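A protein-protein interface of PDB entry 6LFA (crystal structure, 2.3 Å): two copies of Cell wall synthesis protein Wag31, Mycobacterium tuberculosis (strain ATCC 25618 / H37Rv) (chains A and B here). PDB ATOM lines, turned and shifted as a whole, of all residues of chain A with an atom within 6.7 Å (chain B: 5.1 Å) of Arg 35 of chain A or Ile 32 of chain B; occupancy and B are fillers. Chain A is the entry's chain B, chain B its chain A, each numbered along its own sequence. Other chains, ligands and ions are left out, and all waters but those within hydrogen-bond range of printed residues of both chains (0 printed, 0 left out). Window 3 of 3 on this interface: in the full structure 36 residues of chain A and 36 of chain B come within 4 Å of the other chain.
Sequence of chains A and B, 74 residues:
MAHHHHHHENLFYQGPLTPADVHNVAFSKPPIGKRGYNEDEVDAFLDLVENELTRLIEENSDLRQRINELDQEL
Of the printed residues of chain B, Lys 34 of chain A touches Arg 35 (3.6 Å). Of chain B, only Lys 29, Pro 30, Ile 32, Arg 35 and Gly 36 come within 4 Å of Arg 35 of chain A. Ile 32 of chain B touches just one residue of chain A: Arg 35 (3.3 Å). Of the printed residues of chain A, Arg 35 of chain B touches Pro 30 (2.6 Å), Pro 31 (3.2 Å), Lys 34 (3.6 Å) and Arg 35 (3.7 Å).
O of Lys 29 of chain B is in hydrogen-bond range of ND2 of Asn 38 of chain A, at 3.5 Å. The backbone NH (N) of Gly 36 of chain B is in hydrogen-bond range of the backbone carbonyl oxygen (O) of Arg 35 of chain A. The guanidinium group (NH2) of Arg 35 of chain B lies within hydrogen-bond range of the backbone carbonyl oxygen (O) of Pro 31 of chain A (3.2 Å). The guanidinium group of Arg 35 of chain B sits at hydrogen-bond distance from the backbone carbonyl oxygen of Pro 30 of chain A (2.6 Å). The backbone NH (N) of Tyr 37 of chain B lies within hydrogen-bond range of the backbone carbonyl oxygen (O) of Tyr 37 of chain A (3.0 Å). The backbone carbonyl oxygen (O) of Pro 30 of chain B sits at hydrogen-bond distance from the guanidinium group (NH2) of Arg 35 of chain A (2.5 Å).
CD of Pro 30 of chain A touches O of Gly 36 of chain B (3.1 Å). Pro 30 of chain A touches Tyr 37 of chain B. NE of Arg 35 of chain B touches O of Lys 34 of chain A, at 3.6 Å. NH1 of Arg 35 of chain A touches CB of Lys 29 of chain B, 3.8 Å away. CA of Arg 35 of chain B touches O of Arg 35 of chain A, at 3.7 Å. Gly 36 of chain A touches Lys 29 of chain B. Gly 36 of chain A touches Pro 30 of chain B. O of Tyr 37 of chain B touches CA of Gly 36 of chain A, 3.3 Å away. O of Tyr 37 of chain A touches CA of Gly 36 of chain B, at 3.3 Å. ND2 of Asn 38 of chain A touches CD of Pro 31 of chain B, at 3.7 Å.
Pro 30 of chain A touches Tyr 37 of chain B, but with the chains exchanged Tyr 37 of chain A does not touch Pro 30 of chain B (4.2 Å). Pro 31 of chain A touches Arg 35 of chain B, but with the chains exchanged Arg 35 of chain A does not touch Pro 31 of chain B (4.04 Å). Lys 34 of chain A touches Arg 35 of chain B, but with the chains exchanged Arg 35 of chain A does not touch Lys 34 of chain B (4.6 Å). Arg 35 of chain B touches its own counterpart, Arg 35 of chain A. Positions printed for both chains: 30, 31, 33, 34, 35, 36 and 37. Of the 18 pairs that touch across the chains among the printed residues, 8 have their exchanged pair printed and touching as well.
Among the printed residues, 18 pairs touch across the chains.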
ATOM      1  N   PRO A  30      21.366  10.084  13.221  1.00  0.00           N
ATOM      2  CA  PRO A  30      20.272  10.501  12.337  1.00  0.00           C
ATOM      3  C   PRO A  30      19.962  11.963  12.563  1.00  0.00           C
ATOM      4  O   PRO A  30      20.341  12.542  13.593  1.00  0.00           O
ATOM      5  CB  PRO A  30      19.083   9.608  12.760  1.00  0.00           C
ATOM      6  CG  PRO A  30      19.686   8.479  13.547  1.00  0.00           C
ATOM      7  CD  PRO A  30      20.952   9.024  14.160  1.00  0.00           C
ATOM      8  N   PRO A  31      19.256  12.586  11.637  1.00  0.00           N
ATOM      9  CA  PRO A  31      18.794  13.952  11.881  1.00  0.00           C
ATOM     10  C   PRO A  31      17.980  14.014  13.163  1.00  0.00           C
ATOM     11  O   PRO A  31      17.376  13.026  13.589  1.00  0.00           O
ATOM     12  CB  PRO A  31      17.925  14.259  10.651  1.00  0.00           C
ATOM     13  CG  PRO A  31      18.265  13.235   9.651  1.00  0.00           C
ATOM     14  CD  PRO A  31      18.669  12.017  10.417  1.00  0.00           C
ATOM     15  N   GLY A  33      14.670  14.770  14.944  1.00  0.00           N
ATOM     16  CA  GLY A  33      14.887  13.776  15.970  1.00  0.00           C
ATOM     17  C   GLY A  33      14.382  12.500  15.311  1.00  0.00           C
ATOM     18  O   GLY A  33      13.229  12.105  15.488  1.00  0.00           O
ATOM     19  N   LYS A  34      15.235  11.915  14.474  1.00  0.00           N
ATOM     20  CA  LYS A  34      15.021  10.617  13.853  1.00  0.00           C
ATOM     21  C   LYS A  34      15.757   9.552  14.660  1.00  0.00           C
ATOM     22  O   LYS A  34      16.522   9.849  15.582  1.00  0.00           O
ATOM     23  CB  LYS A  34      15.514  10.622  12.399  1.00  0.00           C
ATOM     24  CG  LYS A  34      14.839  11.654  11.488  1.00  0.00           C
ATOM     25  CD  LYS A  34      13.457  11.203  10.998  1.00  0.00           C
ATOM     26  CE  LYS A  34      12.846  12.246  10.037  1.00  0.00           C
ATOM     27  NZ  LYS A  34      11.383  12.529  10.271  1.00  0.00           N
ATOM     28  N   ARG A  35      15.531   8.297  14.297  1.00  0.00           N
ATOM     29  CA  ARG A  35      16.033   7.191  15.095  1.00  0.00           C
ATOM     30  C   ARG A  35      17.140   6.397  14.420  1.00  0.00           C
ATOM     31  O   ARG A  35      18.103   5.990  15.098  1.00  0.00           O
ATOM     32  CB  ARG A  35      14.874   6.275  15.465  1.00  0.00           C
ATOM     33  CG  ARG A  35      13.940   6.964  16.465  1.00  0.00           C
ATOM     34  CD  ARG A  35      12.929   6.003  17.032  1.00  0.00           C
ATOM     35  NE  ARG A  35      13.587   4.914  17.745  1.00  0.00           N
ATOM     36  CZ  ARG A  35      13.088   3.686  17.854  1.00  0.00           C
ATOM     37  NH1 ARG A  35      11.921   3.384  17.287  1.00  0.00           N
ATOM     38  NH2 ARG A  35      13.770   2.756  18.519  1.00  0.00           N
ATOM     39  N   GLY A  36      17.050   6.197  13.105  1.00  0.00           N
ATOM     40  CA  GLY A  36      18.126   5.558  12.374  1.00  0.00           C
ATOM     41  C   GLY A  36      18.098   4.039  12.461  1.00  0.00           C
ATOM     42  O   GLY A  36      17.110   3.424  12.877  1.00  0.00           O
ATOM     43  N   TYR A  37      19.219   3.438  12.032  1.00  0.00           N
ATOM     44  CA  TYR A  37      19.428   1.988  12.014  1.00  0.00           C
ATOM     45  C   TYR A  37      20.096   1.477  13.291  1.00  0.00           C
ATOM     46  O   TYR A  37      21.125   2.012  13.716  1.00  0.00           O
ATOM     47  CB  TYR A  37      20.320   1.589  10.832  1.00  0.00           C
ATOM     48  CG  TYR A  37      19.713   1.744   9.462  1.00  0.00           C
ATOM     49  CD1 TYR A  37      18.345   1.582   9.228  1.00  0.00           C
ATOM     50  CD2 TYR A  37      20.522   2.029   8.387  1.00  0.00           C
ATOM     51  CE1 TYR A  37      17.830   1.722   7.933  1.00  0.00           C
ATOM     52  CE2 TYR A  37      20.022   2.174   7.127  1.00  0.00           C
ATOM     53  CZ  TYR A  37      18.696   2.010   6.890  1.00  0.00           C
ATOM     54  OH  TYR A  37      18.280   2.177   5.585  1.00  0.00           O
ATOM     55  N   ASN A  38      19.558   0.383  13.843  1.00  0.00           N
ATOM     56  CA  ASN A  38      20.195  -0.368  14.933  1.00  0.00           C
ATOM     57  C   ASN A  38      21.688  -0.578  14.698  1.00  0.00           C
ATOM     58  O   ASN A  38      22.095  -1.121  13.668  1.00  0.00           O
ATOM     59  CB  ASN A  38      19.511  -1.727  15.064  1.00  0.00           C
ATOM     60  CG  ASN A  38      19.973  -2.493  16.279  1.00  0.00           C
ATOM     61  OD1 ASN A  38      21.124  -2.943  16.368  1.00  0.00           O
ATOM     62  ND2 ASN A  38      19.081  -2.645  17.222  1.00  0.00           N
ATOM     63  N   LYS B  29      15.077  -0.560  13.877  1.00  0.00           N
ATOM     64  CA  LYS B  29      15.429   0.661  14.577  1.00  0.00           C
ATOM     65  C   LYS B  29      16.185   0.331  15.864  1.00  0.00           C
ATOM     66  O   LYS B  29      16.251  -0.825  16.308  1.00  0.00           O
ATOM     67  CB  LYS B  29      14.168   1.474  14.870  1.00  0.00           C
ATOM     68  CG  LYS B  29      13.986   2.714  13.989  1.00  0.00           C
ATOM     69  CD  LYS B  29      14.030   2.378  12.506  1.00  0.00           C
ATOM     70  CE  LYS B  29      13.655   3.598  11.662  1.00  0.00           C
ATOM     71  NZ  LYS B  29      13.706   3.323  10.195  1.00  0.00           N
ATOM     72  N   PRO B  30      16.802   1.331  16.481  1.00  0.00           N
ATOM     73  CA  PRO B  30      17.600   1.074  17.673  1.00  0.00           C
ATOM     74  C   PRO B  30      16.712   0.741  18.851  1.00  0.00           C
ATOM     75  O   PRO B  30      15.502   1.029  18.834  1.00  0.00           O
ATOM     76  CB  PRO B  30      18.348   2.399  17.901  1.00  0.00           C
ATOM     77  CG  PRO B  30      18.167   3.201  16.621  1.00  0.00           C
ATOM     78  CD  PRO B  30      16.848   2.751  16.088  1.00  0.00           C
ATOM     79  N   PRO B  31      17.270   0.139  19.894  1.00  0.00           N
ATOM     80  CA  PRO B  31      16.563   0.102  21.178  1.00  0.00           C
ATOM     81  C   PRO B  31      16.129   1.511  21.556  1.00  0.00           C
ATOM     82  O   PRO B  31      16.919   2.456  21.484  1.00  0.00           O
ATOM     83  CB  PRO B  31      17.615  -0.451  22.152  1.00  0.00           C
ATOM     84  CG  PRO B  31      18.675  -1.092  21.294  1.00  0.00           C
ATOM     85  CD  PRO B  31      18.667  -0.317  20.008  1.00  0.00           C
ATOM     86  N   ILE B  32      14.852   1.669  21.915  1.00  0.00           N
ATOM     87  CA  ILE B  32      14.423   2.939  22.487  1.00  0.00           C
ATOM     88  C   ILE B  32      15.066   3.062  23.866  1.00  0.00           C
ATOM     89  O   ILE B  32      15.085   2.093  24.638  1.00  0.00           O
ATOM     90  CB  ILE B  32      12.882   3.035  22.543  1.00  0.00           C
ATOM     91  CG1 ILE B  32      12.395   4.486  22.353  1.00  0.00           C
ATOM     92  CG2 ILE B  32      12.327   2.504  23.873  1.00  0.00           C
ATOM     93  CD1 ILE B  32      12.558   5.040  20.927  1.00  0.00           C
ATOM     94  N   GLY B  33      15.630   4.227  24.188  1.00  0.00           N
ATOM     95  CA  GLY B  33      15.543   5.471  23.440  1.00  0.00           C
ATOM     96  C   GLY B  33      16.932   5.921  23.032  1.00  0.00           C
ATOM     97  O   GLY B  33      17.252   7.120  23.024  1.00  0.00           O
ATOM     98  N   LYS B  34      17.774   4.934  22.729  1.00  0.00           N
ATOM     99  CA  LYS B  34      19.001   5.192  22.000  1.00  0.00           C
ATOM    100  C   LYS B  34      18.679   5.508  20.534  1.00  0.00           C
ATOM    101  O   LYS B  34      17.607   5.176  20.006  1.00  0.00           O
ATOM    102  CB  LYS B  34      19.956   3.994  22.122  1.00  0.00           C
ATOM    103  CG  LYS B  34      21.193   4.085  21.222  1.00  0.00           C
ATOM    104  CD  LYS B  34      22.207   2.960  21.495  1.00  0.00           C
ATOM    105  CE  LYS B  34      22.852   3.111  22.871  1.00  0.00           C
ATOM    106  NZ  LYS B  34      24.217   2.510  22.916  1.00  0.00           N
ATOM    107  N   ARG B  35      19.603   6.207  19.890  1.00  0.00           N
ATOM    108  CA  ARG B  35      19.527   6.474  18.466  1.00  0.00           C
ATOM    109  C   ARG B  35      20.613   5.664  17.782  1.00  0.00           C
ATOM    110  O   ARG B  35      21.560   5.171  18.412  1.00  0.00           O
ATOM    111  CB  ARG B  35      19.702   7.964  18.144  1.00  0.00           C
ATOM    112  CG  ARG B  35      19.026   8.907  19.134  1.00  0.00           C
ATOM    113  CD  ARG B  35      19.602  10.311  19.018  1.00  0.00           C
ATOM    114  NE  ARG B  35      19.201  10.917  17.754  1.00  0.00           N
ATOM    115  CZ  ARG B  35      19.870  11.876  17.130  1.00  0.00           C
ATOM    116  NH1 ARG B  35      21.001  12.363  17.646  1.00  0.00           N
ATOM    117  NH2 ARG B  35      19.397  12.342  15.986  1.00  0.00           N
ATOM    118  N   GLY B  36      20.460   5.517  16.482  1.00  0.00           N
ATOM    119  CA  GLY B  36      21.357   4.640  15.777  1.00  0.00           C
ATOM    120  C   GLY B  36      22.204   5.358  14.771  1.00  0.00           C
ATOM    121  O   GLY B  36      22.591   6.506  14.987  1.00  0.00           O
ATOM    122  N   TYR B  37      22.486   4.680  13.667  1.00  0.00           N
ATOM    123  CA  TYR B  37      23.257   5.242  12.576  1.00  0.00           C
ATOM    124  C   TYR B  37      22.355   5.988  11.596  1.00  0.00           C
ATOM    125  O   TYR B  37      21.216   5.592  11.332  1.00  0.00           O
ATOM    126  CB  TYR B  37      24.013   4.130  11.848  1.00  0.00           C
ATOM    127  CG  TYR B  37      25.096   3.459  12.662  1.00  0.00           C
ATOM    128  CD1 TYR B  37      25.863   4.183  13.588  1.00  0.00           C
ATOM    129  CD2 TYR B  37      25.387   2.121  12.475  1.00  0.00           C
ATOM    130  CE1 TYR B  37      26.886   3.572  14.298  1.00  0.00           C
ATOM    131  CE2 TYR B  37      26.400   1.496  13.188  1.00  0.00           C
ATOM    132  CZ  TYR B  37      27.142   2.229  14.104  1.00  0.00           C
ATOM    133  OH  TYR B  37      28.145   1.621  14.809  1.00  0.00           O
